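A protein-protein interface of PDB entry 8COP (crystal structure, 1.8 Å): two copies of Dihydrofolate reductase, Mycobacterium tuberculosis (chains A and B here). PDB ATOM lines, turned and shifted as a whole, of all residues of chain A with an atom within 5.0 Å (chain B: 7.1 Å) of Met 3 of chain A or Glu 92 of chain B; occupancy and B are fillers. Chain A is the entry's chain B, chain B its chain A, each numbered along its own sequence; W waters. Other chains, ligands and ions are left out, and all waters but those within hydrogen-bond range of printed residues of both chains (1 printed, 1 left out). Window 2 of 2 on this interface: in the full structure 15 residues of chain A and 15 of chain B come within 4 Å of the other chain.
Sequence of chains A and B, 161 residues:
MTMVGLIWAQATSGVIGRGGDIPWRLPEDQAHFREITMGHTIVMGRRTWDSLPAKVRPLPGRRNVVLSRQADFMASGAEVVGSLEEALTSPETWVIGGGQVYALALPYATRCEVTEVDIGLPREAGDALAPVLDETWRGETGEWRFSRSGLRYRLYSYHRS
Met 3 of chain A touches Glu 92 of chain B.
Pro 91 of chain B touches Pro 91 of chain A (CB to O, 3.7 Å).
OE2 of Glu 92 of chain A touches CB of Met 3 of chain B (3.8 Å).
Of chain B, only Glu 92 comes within 4 Å of Met 3 of chain A.
Glu 92 of chain B touches just one residue of chain A: Met 3 (3.2 Å).
Printed residues of chain A within 4 Å of Arg 111 of chain B: Arg 111 (3.3 Å).
Printed residues of chain A within 4 Å of Met 3 of chain B: Glu 92 (3.8 Å).
Printed residues of chain A within 4 Å of Pro 91 of chain B: Pro 91.
Of the printed residues of chain B, Glu 92 of chain A touches Met 3.
Of the 9 printed residues of chain A, 4 touch a printed residue of chain B.
Printed residues of chain A that touch a printed residue of chain B: Met 3, Pro 91, Glu 92 and Arg 111.
Of the 19 printed residues of chain B, 4 touch a printed residue of chain A.
Hydrophobic or aromatic side chains of chain B within 4 Å of the printed part of chain A: Met 3 and Pro 91.
Among the printed residues, 4 pairs touch across the chains.
Among the printed residues, no Asp or Glu carboxylate lies within 4 Å of a Lys or Arg side-chain nitrogen of the other chain.
The backbone NH (N) of Thr 93 of chain B sits at hydrogen-bond distance from the backbone carbonyl oxygen (O) of Met 3 of chain B.
A ring nitrogen (NE2) of His 40 of chain B sits close to the side-chain carboxylate (OE1) of Glu 92 of chain B (3.2 Å).
The backbone NH of Thr 41 of chain B is in hydrogen-bond range of the backbone carbonyl oxygen of Glu 92 of chain B (3.2 Å).
The side-chain sulfur (SD) of Met 3 of chain A sits at hydrogen-bond distance from the backbone NH (N) of Gly 5 of chain A (3.6 Å).
The backbone carbonyl oxygen of Val 4 of chain A lies within hydrogen-bond range of the backbone NH of Arg 111 of chain A (3.4 Å).
The indole nitrogen (NE1) of Trp 94 of chain A lies within hydrogen-bond range of the side-chain carboxylate (OE1) of Glu 92 of chain A (2.9 Å).
NH1 of Arg 111 of chain A sits close to NH1 of Arg 111 of chain B.
Water W1 lies within hydrogen-bond range of the guanidinium group of Arg 111 of chain B and the guanidinium group of Arg 111 of chain A.
Met 3 of chain A touches Glu 92 of chain B, and with the chains exchanged Glu 92 of chain A touches Met 3 of chain B.
Pro 91 of chain B touches its own counterpart, Pro 91 of chain A.
Arg 111 of chain A touches its own counterpart, Arg 111 of chain B.
Positions printed for both chains: 3, 4, 5, 91, 92, 93, 94 and 111.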
ATOM      1  N   MET A   3      -2.947   2.460  -4.424  1.00  0.00           N
ATOM      2  CA  MET A   3      -2.315   1.561  -5.380  1.00  0.00           C
ATOM      3  C   MET A   3      -3.303   1.348  -6.541  1.00  0.00           C
ATOM      4  O   MET A   3      -4.301   0.622  -6.383  1.00  0.00           O
ATOM      5  CB  MET A   3      -1.988   0.208  -4.735  1.00  0.00           C
ATOM      6  CG  MET A   3      -1.057  -0.719  -5.539  1.00  0.00           C
ATOM      7  SD  MET A   3      -1.628  -1.354  -7.124  1.00  0.00           S
ATOM      8  CE  MET A   3      -2.992  -2.387  -6.636  1.00  0.00           C
ATOM      9  N   VAL A   4      -3.060   1.989  -7.688  1.00  0.00           N
ATOM     10  CA  VAL A   4      -3.744   1.626  -8.922  1.00  0.00           C
ATOM     11  C   VAL A   4      -2.851   0.643  -9.655  1.00  0.00           C
ATOM     12  O   VAL A   4      -1.657   0.890  -9.815  1.00  0.00           O
ATOM     13  CB  VAL A   4      -4.022   2.860  -9.798  1.00  0.00           C
ATOM     14  CG1 VAL A   4      -4.606   2.427 -11.142  1.00  0.00           C
ATOM     15  CG2 VAL A   4      -4.944   3.827  -9.090  1.00  0.00           C
ATOM     16  N   GLY A   5      -3.411  -0.466 -10.099  1.00  0.00           N
ATOM     17  CA  GLY A   5      -2.666  -1.407 -10.907  1.00  0.00           C
ATOM     18  C   GLY A   5      -3.362  -1.724 -12.213  1.00  0.00           C
ATOM     19  O   GLY A   5      -4.586  -1.755 -12.305  1.00  0.00           O
ATOM     20  N   PRO A  91      -8.950   0.331  -1.726  1.00  0.00           N
ATOM     21  CA  PRO A  91      -7.524   0.186  -1.412  1.00  0.00           C
ATOM     22  C   PRO A  91      -6.750  -0.426  -2.558  1.00  0.00           C
ATOM     23  O   PRO A  91      -5.543  -0.183  -2.684  1.00  0.00           O
ATOM     24  CB  PRO A  91      -7.531  -0.740  -0.189  1.00  0.00           C
ATOM     25  CG  PRO A  91      -8.936  -0.633   0.362  1.00  0.00           C
ATOM     26  CD  PRO A  91      -9.802  -0.466  -0.825  1.00  0.00           C
ATOM     27  N   GLU A  92      -7.427  -1.207  -3.401  1.00  0.00           N
ATOM     28  CA  GLU A  92      -6.826  -1.921  -4.519  1.00  0.00           C
ATOM     29  C   GLU A  92      -7.801  -1.841  -5.690  1.00  0.00           C
ATOM     30  O   GLU A  92      -8.887  -2.432  -5.633  1.00  0.00           O
ATOM     31  CB  GLU A  92      -6.538  -3.368  -4.123  1.00  0.00           C
ATOM     32  CG  GLU A  92      -5.391  -4.000  -4.853  1.00  0.00           C
ATOM     33  CD  GLU A  92      -4.883  -5.267  -4.186  1.00  0.00           C
ATOM     34  OE1 GLU A  92      -4.710  -6.288  -4.888  1.00  0.00           O
ATOM     35  OE2 GLU A  92      -4.651  -5.243  -2.950  1.00  0.00           O
ATOM     36  N   THR A  93      -7.443  -1.071  -6.723  1.00  0.00           N
ATOM     37  CA  THR A  93      -8.189  -1.006  -7.976  1.00  0.00           C
ATOM     38  C   THR A  93      -7.325  -1.604  -9.076  1.00  0.00           C
ATOM     39  O   THR A  93      -6.152  -1.230  -9.215  1.00  0.00           O
ATOM     40  CB  THR A  93      -8.564   0.429  -8.358  1.00  0.00           C
ATOM     41  OG1 THR A  93      -9.340   1.051  -7.326  1.00  0.00           O
ATOM     42  CG2 THR A  93      -9.378   0.419  -9.626  1.00  0.00           C
ATOM     43  N   TRP A  94      -7.900  -2.531  -9.848  1.00  0.00           N
ATOM     44  CA  TRP A  94      -7.197  -3.192 -10.939  1.00  0.00           C
ATOM     45  C   TRP A  94      -7.913  -2.891 -12.244  1.00  0.00           C
ATOM     46  O   TRP A  94      -9.080  -3.261 -12.413  1.00  0.00           O
ATOM     47  CB  TRP A  94      -7.112  -4.701 -10.721  1.00  0.00           C
ATOM     48  CG  TRP A  94      -6.148  -5.056  -9.642  1.00  0.00           C
ATOM     49  CD1 TRP A  94      -6.448  -5.413  -8.357  1.00  0.00           C
ATOM     50  CD2 TRP A  94      -4.723  -4.994  -9.722  1.00  0.00           C
ATOM     51  NE1 TRP A  94      -5.295  -5.621  -7.653  1.00  0.00           N
ATOM     52  CE2 TRP A  94      -4.222  -5.366  -8.465  1.00  0.00           C
ATOM     53  CE3 TRP A  94      -3.820  -4.678 -10.744  1.00  0.00           C
ATOM     54  CZ2 TRP A  94      -2.858  -5.438  -8.201  1.00  0.00           C
ATOM     55  CZ3 TRP A  94      -2.464  -4.759 -10.482  1.00  0.00           C
ATOM     56  CH2 TRP A  94      -1.999  -5.130  -9.220  1.00  0.00           C
ATOM     57  N   THR A 110       0.571   2.621 -10.279  1.00  0.00           N
ATOM     58  CA  THR A 110       1.809   2.412  -9.555  1.00  0.00           C
ATOM     59  C   THR A 110       2.356   1.025  -9.801  1.00  0.00           C
ATOM     60  O   THR A 110       3.500   0.752  -9.426  1.00  0.00           O
ATOM     61  CB  THR A 110       1.597   2.611  -8.048  1.00  0.00           C
ATOM     62  OG1 THR A 110       2.849   2.521  -7.368  1.00  0.00           O
ATOM     63  CG2 THR A 110       0.694   1.528  -7.524  1.00  0.00           C
ATOM     64  N   ARG A 111       1.575   0.164 -10.459  1.00  0.00           N
ATOM     65  CA  ARG A 111       1.854  -1.253 -10.630  1.00  0.00           C
ATOM     66  C   ARG A 111       1.296  -1.701 -11.971  1.00  0.00           C
ATOM     67  O   ARG A 111       0.176  -1.343 -12.327  1.00  0.00           O
ATOM     68  CB  ARG A 111       1.198  -2.079  -9.518  1.00  0.00           C
ATOM     69  CG  ARG A 111       2.081  -2.482  -8.369  1.00  0.00           C
ATOM     70  CD  ARG A 111       1.279  -3.356  -7.441  1.00  0.00           C
ATOM     71  NE  ARG A 111       1.406  -4.754  -7.812  1.00  0.00           N
ATOM     72  CZ  ARG A 111       0.775  -5.750  -7.204  1.00  0.00           C
ATOM     73  NH1 ARG A 111      -0.039  -5.499  -6.190  1.00  0.00           N
ATOM     74  NH2 ARG A 111       0.959  -6.995  -7.618  1.00  0.00           N
ATOM     75  N   MET B   3      -3.667  -3.187   1.268  1.00  0.00           N
ATOM     76  CA  MET B   3      -2.880  -4.396   1.033  1.00  0.00           C
ATOM     77  C   MET B   3      -1.861  -4.542   2.184  1.00  0.00           C
ATOM     78  O   MET B   3      -1.346  -3.525   2.677  1.00  0.00           O
ATOM     79  CB  MET B   3      -2.112  -4.283  -0.281  1.00  0.00           C
ATOM     80  CG  MET B   3      -1.289  -5.500  -0.730  1.00  0.00           C
ATOM     81  SD  MET B   3       0.340  -5.709   0.004  1.00  0.00           S
ATOM     82  CE  MET B   3       1.255  -4.412  -0.783  1.00  0.00           C
ATOM     83  N   VAL B   4      -1.533  -5.782   2.565  1.00  0.00           N
ATOM     84  CA  VAL B   4      -0.463  -6.056   3.512  1.00  0.00           C
ATOM     85  C   VAL B   4       0.456  -7.074   2.866  1.00  0.00           C
ATOM     86  O   VAL B   4       0.043  -8.203   2.586  1.00  0.00           O
ATOM     87  CB  VAL B   4      -0.970  -6.598   4.850  1.00  0.00           C
ATOM     88  CG1 VAL B   4       0.189  -7.261   5.633  1.00  0.00           C
ATOM     89  CG2 VAL B   4      -1.635  -5.515   5.648  1.00  0.00           C
ATOM     90  N   GLY B   5       1.695  -6.685   2.626  1.00  0.00           N
ATOM     91  CA  GLY B   5       2.672  -7.575   2.051  1.00  0.00           C
ATOM     92  C   GLY B   5       3.816  -7.786   3.015  1.00  0.00           C
ATOM     93  O   GLY B   5       4.101  -6.941   3.861  1.00  0.00           O
ATOM     94  N   ILE B  36      10.222  -1.763  -3.510  1.00  0.00           N
ATOM     95  CA  ILE B  36       8.952  -2.293  -3.029  1.00  0.00           C
ATOM     96  C   ILE B  36       8.383  -1.403  -1.932  1.00  0.00           C
ATOM     97  O   ILE B  36       7.190  -1.060  -1.926  1.00  0.00           O
ATOM     98  CB  ILE B  36       9.155  -3.735  -2.528  1.00  0.00           C
ATOM     99  CG1 ILE B  36       9.600  -4.648  -3.678  1.00  0.00           C
ATOM    100  CG2 ILE B  36       7.897  -4.245  -1.811  1.00  0.00           C
ATOM    101  CD1 ILE B  36       8.686  -4.605  -4.886  1.00  0.00           C
ATOM    102  N   THR B  37       9.229  -0.993  -0.999  1.00  0.00           N
ATOM    103  CA  THR B  37       8.722  -0.380   0.213  1.00  0.00           C
ATOM    104  C   THR B  37       8.552   1.120   0.104  1.00  0.00           C
ATOM    105  O   THR B  37       7.761   1.691   0.858  1.00  0.00           O
ATOM    106  CB  THR B  37       9.664  -0.674   1.384  1.00  0.00           C
ATOM    107  OG1 THR B  37      11.001  -0.307   1.016  1.00  0.00           O
ATOM    108  CG2 THR B  37       9.638  -2.151   1.721  1.00  0.00           C
ATOM    109  N   MET B  38       9.297   1.780  -0.774  1.00  0.00           N
ATOM    110  CA  MET B  38       9.368   3.237  -0.726  1.00  0.00           C
ATOM    111  C   MET B  38       7.987   3.874  -0.800  1.00  0.00           C
ATOM    112  O   MET B  38       7.139   3.470  -1.596  1.00  0.00           O
ATOM    113  CB  MET B  38      10.233   3.752  -1.860  1.00  0.00           C
ATOM    114  CG  MET B  38      10.334   5.237  -1.904  1.00  0.00           C
ATOM    115  SD  MET B  38      10.963   5.909  -0.373  1.00  0.00           S
ATOM    116  CE  MET B  38      12.539   5.093  -0.333  1.00  0.00           C
ATOM    117  N   GLY B  39       7.763   4.868   0.060  1.00  0.00           N
ATOM    118  CA  GLY B  39       6.548   5.648   0.081  1.00  0.00           C
ATOM    119  C   GLY B  39       5.420   5.057   0.875  1.00  0.00           C
ATOM    120  O   GLY B  39       4.472   5.782   1.202  1.00  0.00           O
ATOM    121  N   HIS B  40       5.490   3.764   1.203  1.00  0.00           N
ATOM    122  CA  HIS B  40       4.428   3.057   1.901  1.00  0.00           C
ATOM    123  C   HIS B  40       4.742   2.936   3.398  1.00  0.00           C
ATOM    124  O   HIS B  40       5.754   3.430   3.894  1.00  0.00           O
ATOM    125  CB  HIS B  40       4.219   1.680   1.274  1.00  0.00           C
ATOM    126  CG  HIS B  40       4.055   1.702  -0.217  1.00  0.00           C
ATOM    127  ND1 HIS B  40       3.108   2.473  -0.855  1.00  0.00           N
ATOM    128  CD2 HIS B  40       4.709   1.028  -1.192  1.00  0.00           C
ATOM    129  CE1 HIS B  40       3.191   2.276  -2.159  1.00  0.00           C
ATOM    130  NE2 HIS B  40       4.152   1.402  -2.391  1.00  0.00           N
ATOM    131  N   THR B  41       3.844   2.279   4.133  1.00  0.00           N
ATOM    132  CA  THR B  41       4.096   2.023   5.545  1.00  0.00           C
ATOM    133  C   THR B  41       5.009   0.812   5.664  1.00  0.00           C
ATOM    134  O   THR B  41       4.771  -0.210   5.012  1.00  0.00           O
ATOM    135  CB  THR B  41       2.795   1.767   6.307  1.00  0.00           C
ATOM    136  OG1 THR B  41       1.933   2.912   6.234  1.00  0.00           O
ATOM    137  CG2 THR B  41       3.105   1.503   7.773  1.00  0.00           C
ATOM    138  N   ILE B  42       6.072   0.927   6.463  1.00  0.00           N
ATOM    139  CA  ILE B  42       6.895  -0.226   6.831  1.00  0.00           C
ATOM    140  C   ILE B  42       6.690  -0.519   8.311  1.00  0.00           C
ATOM    141  O   ILE B  42       6.690   0.398   9.142  1.00  0.00           O
ATOM    142  CB  ILE B  42       8.388  -0.019   6.523  1.00  0.00           C
ATOM    143  CG1 ILE B  42       8.957   1.131   7.331  1.00  0.00           C
ATOM    144  CG2 ILE B  42       8.604   0.226   5.044  1.00  0.00           C
ATOM    145  CD1 ILE B  42      10.426   1.197   7.225  1.00  0.00           C
ATOM    146  N   ALA B  87      -1.409  -0.502  13.102  1.00  0.00           N
ATOM    147  CA  ALA B  87      -0.501  -0.058  12.060  1.00  0.00           C
ATOM    148  C   ALA B  87      -1.095  -0.156  10.666  1.00  0.00           C
ATOM    149  O   ALA B  87      -0.355  -0.008   9.688  1.00  0.00           O
ATOM    150  CB  ALA B  87       0.797  -0.865  12.117  1.00  0.00           C
ATOM    151  N   LEU B  88      -2.396  -0.372  10.541  1.00  0.00           N
ATOM    152  CA  LEU B  88      -3.022  -0.527   9.236  1.00  0.00           C
ATOM    153  C   LEU B  88      -3.926   0.662   8.953  1.00  0.00           C
ATOM    154  O   LEU B  88      -5.042   0.730   9.471  1.00  0.00           O
ATOM    155  CB  LEU B  88      -3.817  -1.821   9.133  1.00  0.00           C
ATOM    156  CG  LEU B  88      -2.983  -3.082   9.254  1.00  0.00           C
ATOM    157  CD1 LEU B  88      -3.829  -4.285   9.591  1.00  0.00           C
ATOM    158  CD2 LEU B  88      -2.259  -3.233   7.981  1.00  0.00           C
ATOM    159  N   THR B  89      -3.449   1.577   8.101  1.00  0.00           N
ATOM    160  CA  THR B  89      -4.275   2.645   7.543  1.00  0.00           C
ATOM    161  C   THR B  89      -3.564   3.363   6.401  1.00  0.00           C
ATOM    162  O   THR B  89      -3.744   4.572   6.212  1.00  0.00           O
ATOM    163  CB  THR B  89      -4.700   3.637   8.633  1.00  0.00           C
ATOM    164  OG1 THR B  89      -5.588   4.616   8.069  1.00  0.00           O
ATOM    165  CG2 THR B  89      -3.483   4.298   9.283  1.00  0.00           C
ATOM    166  N   SER B  90      -2.733   2.625   5.662  1.00  0.00           N
ATOM    167  CA  SER B  90      -2.289   2.940   4.312  1.00  0.00           C
ATOM    168  C   SER B  90      -2.736   1.825   3.380  1.00  0.00           C
ATOM    169  O   SER B  90      -2.960   0.694   3.821  1.00  0.00           O
ATOM    170  CB  SER B  90      -0.765   3.119   4.211  1.00  0.00           C
ATOM    171  OG  SER B  90      -0.300   4.235   4.961  1.00  0.00           O
ATOM    172  N   PRO B  91      -2.947   2.122   2.097  1.00  0.00           N
ATOM    173  CA  PRO B  91      -3.290   1.047   1.155  1.00  0.00           C
ATOM    174  C   PRO B  91      -2.172   0.035   0.974  1.00  0.00           C
ATOM    175  O   PRO B  91      -2.452  -1.096   0.544  1.00  0.00           O
ATOM    176  CB  PRO B  91      -3.605   1.786  -0.155  1.00  0.00           C
ATOM    177  CG  PRO B  91      -3.212   3.206   0.022  1.00  0.00           C
ATOM    178  CD  PRO B  91      -2.905   3.460   1.471  1.00  0.00           C
ATOM    179  N   GLU B  92      -0.921   0.391   1.289  1.00  0.00           N
ATOM    180  CA  GLU B  92       0.204  -0.543   1.229  1.00  0.00           C
ATOM    181  C   GLU B  92       0.951  -0.478   2.551  1.00  0.00           C
ATOM    182  O   GLU B  92       1.368   0.604   2.979  1.00  0.00           O
ATOM    183  CB  GLU B  92       1.138  -0.212   0.069  1.00  0.00           C
ATOM    184  CG  GLU B  92       0.552  -0.549  -1.273  1.00  0.00           C
ATOM    185  CD  GLU B  92       1.583  -0.770  -2.351  1.00  0.00           C
ATOM    186  OE1 GLU B  92       2.646  -1.379  -2.103  1.00  0.00           O
ATOM    187  OE2 GLU B  92       1.324  -0.290  -3.468  1.00  0.00           O
ATOM    188  N   THR B  93       1.097  -1.630   3.202  1.00  0.00           N
ATOM    189  CA  THR B  93       1.796  -1.750   4.478  1.00  0.00           C
ATOM    190  C   THR B  93       2.749  -2.926   4.376  1.00  0.00           C
ATOM    191  O   THR B  93       2.327  -4.044   4.071  1.00  0.00           O
ATOM    192  CB  THR B  93       0.821  -1.945   5.656  1.00  0.00           C
ATOM    193  OG1 THR B  93      -0.060  -0.816   5.804  1.00  0.00           O
ATOM    194  CG2 THR B  93       1.573  -2.143   6.941  1.00  0.00           C
ATOM    195  N   TRP B  94       4.023  -2.692   4.623  1.00  0.00           N
ATOM    196  CA  TRP B  94       5.031  -3.720   4.385  1.00  0.00           C
ATOM    197  C   TRP B  94       5.676  -4.160   5.695  1.00  0.00           C
ATOM    198  O   TRP B  94       6.359  -3.380   6.359  1.00  0.00           O
ATOM    199  CB  TRP B  94       6.073  -3.235   3.378  1.00  0.00           C
ATOM    200  CG  TRP B  94       5.524  -3.236   1.989  1.00  0.00           C
ATOM    201  CD1 TRP B  94       5.052  -2.159   1.296  1.00  0.00           C
ATOM    202  CD2 TRP B  94       5.381  -4.368   1.122  1.00  0.00           C
ATOM    203  NE1 TRP B  94       4.624  -2.555   0.057  1.00  0.00           N
ATOM    204  CE2 TRP B  94       4.816  -3.905  -0.075  1.00  0.00           C
ATOM    205  CE3 TRP B  94       5.681  -5.728   1.243  1.00  0.00           C
ATOM    206  CZ2 TRP B  94       4.543  -4.753  -1.146  1.00  0.00           C
ATOM    207  CZ3 TRP B  94       5.411  -6.565   0.182  1.00  0.00           C
ATOM    208  CH2 TRP B  94       4.847  -6.073  -1.001  1.00  0.00           C
ATOM    209  N   ARG B 111       0.500 -10.464  -0.083  1.00  0.00           N
ATOM    210  CA  ARG B 111       1.714 -10.496  -0.884  1.00  0.00           C
ATOM    211  C   ARG B 111       2.898 -10.895  -0.006  1.00  0.00           C
ATOM    212  O   ARG B 111       3.005 -10.456   1.142  1.00  0.00           O
ATOM    213  CB  ARG B 111       1.980  -9.133  -1.515  1.00  0.00           C
ATOM    214  CG  ARG B 111       1.148  -8.900  -2.760  1.00  0.00           C
ATOM    215  CD  ARG B 111       1.440  -7.563  -3.424  1.00  0.00           C
ATOM    216  NE  ARG B 111       2.685  -7.597  -4.189  1.00  0.00           N
ATOM    217  CZ  ARG B 111       3.267  -6.527  -4.724  1.00  0.00           C
ATOM    218  NH1 ARG B 111       2.758  -5.322  -4.523  1.00  0.00           N
ATOM    219  NH2 ARG B 111       4.383  -6.669  -5.420  1.00  0.00           N
HETATM  220  O   HOH W   1       3.006  -8.932  -6.596  1.00  0.00           O
